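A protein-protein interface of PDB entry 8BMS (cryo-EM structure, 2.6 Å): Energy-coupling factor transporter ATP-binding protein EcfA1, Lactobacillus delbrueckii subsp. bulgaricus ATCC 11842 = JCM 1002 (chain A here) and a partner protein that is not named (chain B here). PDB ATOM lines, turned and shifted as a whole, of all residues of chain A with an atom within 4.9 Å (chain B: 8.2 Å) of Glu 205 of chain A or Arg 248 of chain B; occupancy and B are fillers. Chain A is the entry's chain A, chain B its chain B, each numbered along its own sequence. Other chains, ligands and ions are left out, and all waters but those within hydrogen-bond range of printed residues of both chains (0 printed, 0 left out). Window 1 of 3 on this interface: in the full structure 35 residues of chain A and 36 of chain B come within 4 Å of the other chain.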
ATOM      1  N   ASP A 203     -16.729   7.362  22.778  1.00  0.00           N
ATOM      2  CA  ASP A 203     -17.035   6.149  23.523  1.00  0.00           C
ATOM      3  C   ASP A 203     -17.982   5.290  22.695  1.00  0.00           C
ATOM      4  O   ASP A 203     -19.120   5.693  22.428  1.00  0.00           O
ATOM      5  CB  ASP A 203     -17.657   6.491  24.876  1.00  0.00           C
ATOM      6  CG  ASP A 203     -17.729   5.297  25.806  1.00  0.00           C
ATOM      7  OD1 ASP A 203     -17.122   4.254  25.487  1.00  0.00           O
ATOM      8  OD2 ASP A 203     -18.394   5.402  26.856  1.00  0.00           O
ATOM      9  N   LEU A 204     -17.513   4.112  22.290  1.00  0.00           N
ATOM     10  CA  LEU A 204     -18.306   3.250  21.424  1.00  0.00           C
ATOM     11  C   LEU A 204     -19.386   2.486  22.176  1.00  0.00           C
ATOM     12  O   LEU A 204     -20.333   2.006  21.548  1.00  0.00           O
ATOM     13  CB  LEU A 204     -17.391   2.274  20.689  1.00  0.00           C
ATOM     14  CG  LEU A 204     -16.240   2.950  19.944  1.00  0.00           C
ATOM     15  CD1 LEU A 204     -15.155   1.947  19.637  1.00  0.00           C
ATOM     16  CD2 LEU A 204     -16.738   3.614  18.671  1.00  0.00           C
ATOM     17  N   GLU A 205     -19.269   2.365  23.499  1.00  0.00           N
ATOM     18  CA  GLU A 205     -20.352   1.771  24.277  1.00  0.00           C
ATOM     19  C   GLU A 205     -21.596   2.649  24.240  1.00  0.00           C
ATOM     20  O   GLU A 205     -22.720   2.143  24.148  1.00  0.00           O
ATOM     21  CB  GLU A 205     -19.899   1.536  25.715  1.00  0.00           C
ATOM     22  CG  GLU A 205     -18.542   0.863  25.834  1.00  0.00           C
ATOM     23  CD  GLU A 205     -18.496  -0.484  25.142  1.00  0.00           C
ATOM     24  OE1 GLU A 205     -19.502  -1.221  25.206  1.00  0.00           O
ATOM     25  OE2 GLU A 205     -17.455  -0.806  24.534  1.00  0.00           O
ATOM     26  N   GLU A 206     -21.412   3.968  24.319  1.00  0.00           N
ATOM     27  CA  GLU A 206     -22.536   4.886  24.180  1.00  0.00           C
ATOM     28  C   GLU A 206     -23.076   4.885  22.755  1.00  0.00           C
ATOM     29  O   GLU A 206     -24.293   4.965  22.545  1.00  0.00           O
ATOM     30  CB  GLU A 206     -22.112   6.293  24.598  1.00  0.00           C
ATOM     31  CG  GLU A 206     -23.156   7.364  24.344  1.00  0.00           C
ATOM     32  CD  GLU A 206     -22.680   8.742  24.747  1.00  0.00           C
ATOM     33  OE1 GLU A 206     -21.575   8.845  25.319  1.00  0.00           O
ATOM     34  OE2 GLU A 206     -23.408   9.723  24.489  1.00  0.00           O
ATOM     35  N   ALA A 207     -22.187   4.797  21.762  1.00  0.00           N
ATOM     36  CA  ALA A 207     -22.627   4.784  20.372  1.00  0.00           C
ATOM     37  C   ALA A 207     -23.407   3.521  20.036  1.00  0.00           C
ATOM     38  O   ALA A 207     -24.323   3.564  19.207  1.00  0.00           O
ATOM     39  CB  ALA A 207     -21.425   4.928  19.439  1.00  0.00           C
ATOM     40  N   ALA A 208     -23.060   2.393  20.658  1.00  0.00           N
ATOM     41  CA  ALA A 208     -23.770   1.146  20.397  1.00  0.00           C
ATOM     42  C   ALA A 208     -25.211   1.183  20.886  1.00  0.00           C
ATOM     43  O   ALA A 208     -26.050   0.448  20.354  1.00  0.00           O
ATOM     44  CB  ALA A 208     -23.029  -0.023  21.047  1.00  0.00           C
ATOM     45  N   GLY A 209     -25.516   2.012  21.878  1.00  0.00           N
ATOM     46  CA  GLY A 209     -26.861   2.167  22.385  1.00  0.00           C
ATOM     47  C   GLY A 209     -27.680   3.246  21.715  1.00  0.00           C
ATOM     48  O   GLY A 209     -28.793   3.532  22.169  1.00  0.00           O
ATOM     49  N   PRO A 245     -17.344  -1.879  19.970  1.00  0.00           N
ATOM     50  CA  PRO A 245     -17.624  -1.928  21.413  1.00  0.00           C
ATOM     51  C   PRO A 245     -17.204  -3.230  22.081  1.00  0.00           C
ATOM     52  O   PRO A 245     -16.663  -4.134  21.436  1.00  0.00           O
ATOM     53  CB  PRO A 245     -19.146  -1.729  21.490  1.00  0.00           C
ATOM     54  CG  PRO A 245     -19.654  -1.906  20.106  1.00  0.00           C
ATOM     55  CD  PRO A 245     -18.544  -1.552  19.184  1.00  0.00           C
ATOM     56  N   PHE A 246     -17.462  -3.318  23.389  1.00  0.00           N
ATOM     57  CA  PHE A 246     -16.930  -4.408  24.201  1.00  0.00           C
ATOM     58  C   PHE A 246     -17.427  -5.770  23.726  1.00  0.00           C
ATOM     59  O   PHE A 246     -16.651  -6.731  23.658  1.00  0.00           O
ATOM     60  CB  PHE A 246     -17.305  -4.177  25.667  1.00  0.00           C
ATOM     61  CG  PHE A 246     -16.995  -5.337  26.573  1.00  0.00           C
ATOM     62  CD1 PHE A 246     -15.728  -5.498  27.104  1.00  0.00           C
ATOM     63  CD2 PHE A 246     -17.978  -6.253  26.911  1.00  0.00           C
ATOM     64  CE1 PHE A 246     -15.441  -6.558  27.939  1.00  0.00           C
ATOM     65  CE2 PHE A 246     -17.697  -7.315  27.747  1.00  0.00           C
ATOM     66  CZ  PHE A 246     -16.427  -7.468  28.262  1.00  0.00           C
ATOM     67  N   ARG A 249     -15.723  -7.105  20.474  1.00  0.00           N
ATOM     68  CA  ARG A 249     -14.356  -7.525  20.760  1.00  0.00           C
ATOM     69  C   ARG A 249     -14.337  -8.849  21.515  1.00  0.00           C
ATOM     70  O   ARG A 249     -13.544  -9.741  21.196  1.00  0.00           O
ATOM     71  CB  ARG A 249     -13.624  -6.446  21.556  1.00  0.00           C
ATOM     72  CG  ARG A 249     -13.543  -5.102  20.863  1.00  0.00           C
ATOM     73  CD  ARG A 249     -12.681  -4.127  21.644  1.00  0.00           C
ATOM     74  NE  ARG A 249     -13.241  -3.837  22.959  1.00  0.00           N
ATOM     75  CZ  ARG A 249     -12.992  -2.735  23.653  1.00  0.00           C
ATOM     76  NH1 ARG A 249     -12.197  -1.787  23.183  1.00  0.00           N
ATOM     77  NH2 ARG A 249     -13.558  -2.579  24.846  1.00  0.00           N
ATOM     78  N   ASP A 268     -24.776  -7.331  25.730  1.00  0.00           N
ATOM     79  CA  ASP A 268     -24.175  -8.134  26.788  1.00  0.00           C
ATOM     80  C   ASP A 268     -25.096  -9.272  27.213  1.00  0.00           C
ATOM     81  O   ASP A 268     -24.639 -10.397  27.444  1.00  0.00           O
ATOM     82  CB  ASP A 268     -23.828  -7.251  27.985  1.00  0.00           C
ATOM     83  CG  ASP A 268     -22.641  -6.348  27.718  1.00  0.00           C
ATOM     84  OD1 ASP A 268     -22.376  -6.046  26.536  1.00  0.00           O
ATOM     85  OD2 ASP A 268     -21.972  -5.940  28.691  1.00  0.00           O
ATOM     86  N   PRO B 178     -10.816   6.010  19.512  1.00  0.00           N
ATOM     87  CA  PRO B 178     -10.432   4.672  20.007  1.00  0.00           C
ATOM     88  C   PRO B 178      -9.048   4.198  19.583  1.00  0.00           C
ATOM     89  O   PRO B 178      -8.265   3.747  20.432  1.00  0.00           O
ATOM     90  CB  PRO B 178     -11.537   3.781  19.433  1.00  0.00           C
ATOM     91  CG  PRO B 178     -12.725   4.665  19.372  1.00  0.00           C
ATOM     92  CD  PRO B 178     -12.230   6.056  19.097  1.00  0.00           C
ATOM     93  N   ASN B 204     -11.343   5.503  33.332  1.00  0.00           N
ATOM     94  CA  ASN B 204     -11.637   4.241  32.665  1.00  0.00           C
ATOM     95  C   ASN B 204     -10.946   3.129  33.442  1.00  0.00           C
ATOM     96  O   ASN B 204      -9.715   3.026  33.426  1.00  0.00           O
ATOM     97  CB  ASN B 204     -11.171   4.279  31.211  1.00  0.00           C
ATOM     98  CG  ASN B 204     -11.662   3.094  30.404  1.00  0.00           C
ATOM     99  OD1 ASN B 204     -12.782   2.621  30.590  1.00  0.00           O
ATOM    100  ND2 ASN B 204     -10.824   2.609  29.497  1.00  0.00           N
ATOM    101  N   MET B 205     -11.736   2.297  34.124  1.00  0.00           N
ATOM    102  CA  MET B 205     -11.168   1.231  34.939  1.00  0.00           C
ATOM    103  C   MET B 205     -10.547   0.124  34.097  1.00  0.00           C
ATOM    104  O   MET B 205      -9.731  -0.647  34.614  1.00  0.00           O
ATOM    105  CB  MET B 205     -12.237   0.647  35.863  1.00  0.00           C
ATOM    106  CG  MET B 205     -12.767   1.630  36.893  1.00  0.00           C
ATOM    107  SD  MET B 205     -11.451   2.502  37.762  1.00  0.00           S
ATOM    108  CE  MET B 205     -11.861   4.203  37.387  1.00  0.00           C
ATOM    109  N   ASP B 206     -10.916   0.028  32.819  1.00  0.00           N
ATOM    110  CA  ASP B 206     -10.270  -0.938  31.937  1.00  0.00           C
ATOM    111  C   ASP B 206      -8.796  -0.606  31.746  1.00  0.00           C
ATOM    112  O   ASP B 206      -7.951  -1.506  31.724  1.00  0.00           O
ATOM    113  CB  ASP B 206     -10.996  -0.987  30.594  1.00  0.00           C
ATOM    114  CG  ASP B 206     -12.457  -1.362  30.738  1.00  0.00           C
ATOM    115  OD1 ASP B 206     -13.243  -0.526  31.228  1.00  0.00           O
ATOM    116  OD2 ASP B 206     -12.820  -2.498  30.362  1.00  0.00           O
ATOM    117  N   ASP B 207      -8.469   0.682  31.617  1.00  0.00           N
ATOM    118  CA  ASP B 207      -7.068   1.086  31.552  1.00  0.00           C
ATOM    119  C   ASP B 207      -6.330   0.710  32.828  1.00  0.00           C
ATOM    120  O   ASP B 207      -5.176   0.266  32.783  1.00  0.00           O
ATOM    121  CB  ASP B 207      -6.967   2.591  31.303  1.00  0.00           C
ATOM    122  CG  ASP B 207      -7.458   2.989  29.928  1.00  0.00           C
ATOM    123  OD1 ASP B 207      -7.680   2.091  29.089  1.00  0.00           O
ATOM    124  OD2 ASP B 207      -7.624   4.203  29.684  1.00  0.00           O
ATOM    125  N   ALA B 209      -7.059  -1.796  34.863  1.00  0.00           N
ATOM    126  CA  ALA B 209      -6.869  -3.242  34.893  1.00  0.00           C
ATOM    127  C   ALA B 209      -5.843  -3.702  33.865  1.00  0.00           C
ATOM    128  O   ALA B 209      -5.196  -4.737  34.060  1.00  0.00           O
ATOM    129  CB  ALA B 209      -8.203  -3.953  34.668  1.00  0.00           C
ATOM    130  N   ALA B 245     -15.856   2.519  40.187  1.00  0.00           N
ATOM    131  CA  ALA B 245     -16.479   1.531  39.321  1.00  0.00           C
ATOM    132  C   ALA B 245     -15.555   0.325  39.161  1.00  0.00           C
ATOM    133  O   ALA B 245     -14.514   0.217  39.811  1.00  0.00           O
ATOM    134  CB  ALA B 245     -16.833   2.153  37.969  1.00  0.00           C
ATOM    135  N   GLU B 246     -15.950  -0.581  38.275  1.00  0.00           N
ATOM    136  CA  GLU B 246     -15.268  -1.842  38.046  1.00  0.00           C
ATOM    137  C   GLU B 246     -15.020  -2.010  36.555  1.00  0.00           C
ATOM    138  O   GLU B 246     -15.798  -1.509  35.737  1.00  0.00           O
ATOM    139  CB  GLU B 246     -16.120  -3.007  38.574  1.00  0.00           C
ATOM    140  CG  GLU B 246     -15.349  -4.239  39.009  1.00  0.00           C
ATOM    141  CD  GLU B 246     -16.254  -5.317  39.569  1.00  0.00           C
ATOM    142  OE1 GLU B 246     -17.489  -5.170  39.460  1.00  0.00           O
ATOM    143  OE2 GLU B 246     -15.731  -6.308  40.119  1.00  0.00           O
ATOM    144  N   PRO B 247     -13.938  -2.690  36.170  1.00  0.00           N
ATOM    145  CA  PRO B 247     -13.686  -2.916  34.743  1.00  0.00           C
ATOM    146  C   PRO B 247     -14.826  -3.680  34.087  1.00  0.00           C
ATOM    147  O   PRO B 247     -15.480  -4.519  34.709  1.00  0.00           O
ATOM    148  CB  PRO B 247     -12.390  -3.731  34.735  1.00  0.00           C
ATOM    149  CG  PRO B 247     -11.710  -3.359  35.995  1.00  0.00           C
ATOM    150  CD  PRO B 247     -12.796  -3.110  37.000  1.00  0.00           C
ATOM    151  N   ARG B 248     -15.064  -3.365  32.810  1.00  0.00           N
ATOM    152  CA  ARG B 248     -16.162  -3.995  32.086  1.00  0.00           C
ATOM    153  C   ARG B 248     -15.985  -5.505  31.991  1.00  0.00           C
ATOM    154  O   ARG B 248     -16.975  -6.239  31.925  1.00  0.00           O
ATOM    155  CB  ARG B 248     -16.293  -3.386  30.691  1.00  0.00           C
ATOM    156  CG  ARG B 248     -17.731  -3.181  30.247  1.00  0.00           C
ATOM    157  CD  ARG B 248     -17.815  -2.283  29.024  1.00  0.00           C
ATOM    158  NE  ARG B 248     -19.164  -1.767  28.820  1.00  0.00           N
ATOM    159  CZ  ARG B 248     -20.152  -2.449  28.256  1.00  0.00           C
ATOM    160  NH1 ARG B 248     -19.978  -3.688  27.826  1.00  0.00           N
ATOM    161  NH2 ARG B 248     -21.343  -1.874  28.122  1.00  0.00           N
ATOM    162  N   SER B 249     -14.740  -5.986  31.981  1.00  0.00           N
ATOM    163  CA  SER B 249     -14.513  -7.427  32.001  1.00  0.00           C
ATOM    164  C   SER B 249     -14.990  -8.041  33.312  1.00  0.00           C
ATOM    165  O   SER B 249     -15.631  -9.099  33.312  1.00  0.00           O
ATOM    166  CB  SER B 249     -13.035  -7.729  31.770  1.00  0.00           C
ATOM    167  OG  SER B 249     -12.606  -7.224  30.518  1.00  0.00           O
ATOM    168  N   ALA B 250     -14.697  -7.387  34.439  1.00  0.00           N
ATOM    169  CA  ALA B 250     -15.176  -7.877  35.726  1.00  0.00           C
ATOM    170  C   ALA B 250     -16.696  -7.806  35.816  1.00  0.00           C
ATOM    171  O   ALA B 250     -17.334  -8.710  36.368  1.00  0.00           O
ATOM    172  CB  ALA B 250     -14.531  -7.086  36.862  1.00  0.00           C
ATOM    173  N   ARG B 251     -17.292  -6.737  35.285  1.00  0.00           N
ATOM    174  CA  ARG B 251     -18.749  -6.627  35.280  1.00  0.00           C
ATOM    175  C   ARG B 251     -19.381  -7.729  34.437  1.00  0.00           C
ATOM    176  O   ARG B 251     -20.400  -8.311  34.827  1.00  0.00           O
ATOM    177  CB  ARG B 251     -19.167  -5.249  34.773  1.00  0.00           C
ATOM    178  CG  ARG B 251     -18.929  -4.128  35.772  1.00  0.00           C
ATOM    179  CD  ARG B 251     -18.800  -2.782  35.081  1.00  0.00           C
ATOM    180  NE  ARG B 251     -19.889  -2.537  34.144  1.00  0.00           N
ATOM    181  CZ  ARG B 251     -19.845  -1.649  33.161  1.00  0.00           C
ATOM    182  NH1 ARG B 251     -18.776  -0.897  32.957  1.00  0.00           N
ATOM    183  NH2 ARG B 251     -20.900  -1.512  32.364  1.00  0.00           N
ATOM    184  N   PHE B 252     -18.789  -8.030  33.280  1.00  0.00           N
ATOM    185  CA  PHE B 252     -19.307  -9.113  32.451  1.00  0.00           C
ATOM    186  C   PHE B 252     -19.129 -10.463  33.132  1.00  0.00           C
ATOM    187  O   PHE B 252     -19.986 -11.344  33.003  1.00  0.00           O
ATOM    188  CB  PHE B 252     -18.627  -9.108  31.083  1.00  0.00           C
ATOM    189  CG  PHE B 252     -19.290 -10.005  30.078  1.00  0.00           C
ATOM    190  CD1 PHE B 252     -20.321  -9.533  29.284  1.00  0.00           C
ATOM    191  CD2 PHE B 252     -18.885 -11.321  29.929  1.00  0.00           C
ATOM    192  CE1 PHE B 252     -20.935 -10.355  28.362  1.00  0.00           C
ATOM    193  CE2 PHE B 252     -19.496 -12.148  29.008  1.00  0.00           C
ATOM    194  CZ  PHE B 252     -20.522 -11.665  28.223  1.00  0.00           C
ATOM    195  N   ALA B 253     -18.020 -10.652  33.851  1.00  0.00           N
ATOM    196  CA  ALA B 253     -17.837 -11.886  34.608  1.00  0.00           C
ATOM    197  C   ALA B 253     -18.893 -12.023  35.697  1.00  0.00           C
ATOM    198  O   ALA B 253     -19.415 -13.119  35.935  1.00  0.00           O
ATOM    199  CB  ALA B 253     -16.432 -11.932  35.209  1.00  0.00           C
ATOM    200  N   ALA B 254     -19.218 -10.918  36.372  1.00  0.00           N
ATOM    201  CA  ALA B 254     -20.282 -10.944  37.371  1.00  0.00           C
ATOM    202  C   ALA B 254     -21.627 -11.275  36.735  1.00  0.00           C
ATOM    203  O   ALA B 254     -22.413 -12.051  37.294  1.00  0.00           O
ATOM    204  CB  ALA B 254     -20.350  -9.605  38.104  1.00  0.00           C
ATOM    205  N   LYS B 255     -21.910 -10.693  35.567  1.00  0.00           N
ATOM    206  CA  LYS B 255     -23.147 -11.012  34.857  1.00  0.00           C
ATOM    207  C   LYS B 255     -23.201 -12.487  34.481  1.00  0.00           C
ATOM    208  O   LYS B 255     -24.246 -13.134  34.618  1.00  0.00           O
ATOM    209  CB  LYS B 255     -23.277 -10.145  33.605  1.00  0.00           C
ATOM    210  CG  LYS B 255     -23.472  -8.665  33.869  1.00  0.00           C
ATOM    211  CD  LYS B 255     -23.838  -7.934  32.588  1.00  0.00           C
ATOM    212  CE  LYS B 255     -23.352  -6.495  32.612  1.00  0.00           C
ATOM    213  NZ  LYS B 255     -24.456  -5.532  32.359  1.00  0.00           N
ATOM    214  N   PRO B 267     -11.562 -12.374  36.521  1.00  0.00           N
ATOM    215  CA  PRO B 267     -11.016 -11.687  35.347  1.00  0.00           C
ATOM    216  C   PRO B 267     -11.153 -10.176  35.473  1.00  0.00           C
ATOM    217  O   PRO B 267     -12.145  -9.663  35.994  1.00  0.00           O
ATOM    218  CB  PRO B 267     -11.864 -12.232  34.192  1.00  0.00           C
ATOM    219  CG  PRO B 267     -12.407 -13.528  34.696  1.00  0.00           C
ATOM    220  CD  PRO B 267     -12.627 -13.324  36.162  1.00  0.00           C
ATOM    221  N   LEU B 268     -10.137  -9.466  34.988  1.00  0.00           N
ATOM    222  CA  LEU B 268     -10.163  -8.010  34.926  1.00  0.00           C
ATOM    223  C   LEU B 268      -9.840  -7.453  33.550  1.00  0.00           C
ATOM    224  O   LEU B 268     -10.236  -6.318  33.261  1.00  0.00           O
ATOM    225  CB  LEU B 268      -9.185  -7.407  35.945  1.00  0.00           C
ATOM    226  CG  LEU B 268      -9.499  -7.657  37.421  1.00  0.00           C
ATOM    227  CD1 LEU B 268      -8.311  -7.292  38.291  1.00  0.00           C
ATOM    228  CD2 LEU B 268     -10.733  -6.884  37.845  1.00  0.00           C
ATOM    229  N   THR B 269      -9.143  -8.199  32.701  1.00  0.00           N
ATOM    230  CA  THR B 269      -8.851  -7.799  31.335  1.00  0.00           C
ATOM    231  C   THR B 269      -9.624  -8.685  30.366  1.00  0.00           C
ATOM    232  O   THR B 269     -10.044  -9.794  30.704  1.00  0.00           O
ATOM    233  CB  THR B 269      -7.349  -7.883  31.044  1.00  0.00           C
ATOM    234  OG1 THR B 269      -6.946  -9.255  30.987  1.00  0.00           O
ATOM    235  CG2 THR B 269      -6.559  -7.179  32.134  1.00  0.00           C
ATOM    236  N   MET B 270      -9.816  -8.172  29.151  1.00  0.00           N
ATOM    237  CA  MET B 270     -10.602  -8.900  28.157  1.00  0.00           C
ATOM    238  C   MET B 270      -9.996 -10.249  27.782  1.00  0.00           C
ATOM    239  O   MET B 270     -10.743 -11.243  27.748  1.00  0.00           O
ATOM    240  CB  MET B 270     -10.809  -8.020  26.922  1.00  0.00           C
ATOM    241  CG  MET B 270     -11.715  -8.634  25.874  1.00  0.00           C
ATOM    242  SD  MET B 270     -11.922  -7.547  24.458  1.00  0.00           S
ATOM    243  CE  MET B 270     -12.957  -6.277  25.172  1.00  0.00           C
ATOM    244  N   LEU B 273     -10.708 -12.580  30.621  1.00  0.00           N
ATOM    245  CA  LEU B 273     -12.106 -12.995  30.647  1.00  0.00           C
ATOM    246  C   LEU B 273     -12.391 -14.038  29.576  1.00  0.00           C
ATOM    247  O   LEU B 273     -13.136 -14.995  29.815  1.00  0.00           O
ATOM    248  CB  LEU B 273     -13.015 -11.779  30.474  1.00  0.00           C
ATOM    249  CG  LEU B 273     -14.490 -12.049  30.172  1.00  0.00           C
ATOM    250  CD1 LEU B 273     -15.181 -12.661  31.378  1.00  0.00           C
ATOM    251  CD2 LEU B 273     -15.187 -10.769  29.748  1.00  0.00           C
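The guanidinium group of Arg 248 of chain B is in salt-bridge range of the side-chain carboxylate of Glu 205 of chain A, 3.5 Å away.
NH1 of Arg 248 of chain B lies within salt-bridge range of OD2 of Asp 268 of chain A, 3.1 Å away.
OD1 of Asp 203 of chain A lies close to N of Glu 205 of chain A (3.5 Å).
The backbone NH of Phe 246 of chain A is in hydrogen-bond range of the side-chain carboxylate of Glu 205 of chain A (2.8 Å).
The backbone NH (N) of Arg 248 of chain B lies within hydrogen-bond range of the side-chain carboxylate (OD2) of Asp 206 of chain B (3.4 Å).
The side-chain hydroxyl (OG) of Ser 249 of chain B lies within hydrogen-bond range of the backbone NH (N) of Met 270 of chain B (3.2 Å).
Among the printed residues, merely in contact across the chains: Arg 249 of chain A with Met 270 of chain B (3.3 Å), Phe 246 of chain A with Arg 248 of chain B (3.4 Å), Phe 246 of chain A with Met 270 of chain B (3.5 Å), Leu 204 of chain A with Pro 178 of chain B (3.7 Å), Phe 246 of chain A with Phe 252 of chain B (3.8 Å), Asp 268 of chain A with Phe 252 of chain B (3.8 Å), Phe 246 of chain A with Leu 273 of chain B (3.8 Å) and Phe 246 of chain A with Ser 249 of chain B (3.9 Å).
Printed residues of chain B within 4 Å of Leu 204 of chain A: Pro 178 (3.7 Å).
Glu 205 of chain A touches one residue of chain B.
Printed residues of chain B within 4 Å of Phe 246 of chain A: Arg 248, Ser 249, Phe 252, Met 270 and Leu 273.
Ala 209 of chain B touches none of the printed residues of chain A.
Of chain A, only Glu 205, Phe 246 and Asp 268 come within 4 Å of Arg 248 of chain B.
Printed residues of chain A within 4 Å of Phe 252 of chain B: Phe 246 (3.8 Å) and Asp 268 (3.8 Å).
The nearest printed residue of chain A that does not touch Arg 248 of chain B is Arg 249 of chain A (6.0 Å).
The nearest printed residue of chain A that does not touch Met 270 of chain B is Pro 245 of chain A (5.7 Å).
Of the 22 printed residues of chain B, 6 touch a printed residue of chain A.
Of the 11 printed residues of chain A, 5 touch a printed residue of chain B.
Hydrophobic or aromatic side chains of chain A that line the printed part of chain B: Leu 204 and Phe 246.
Among the printed residues, 10 pairs touch across the chains.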
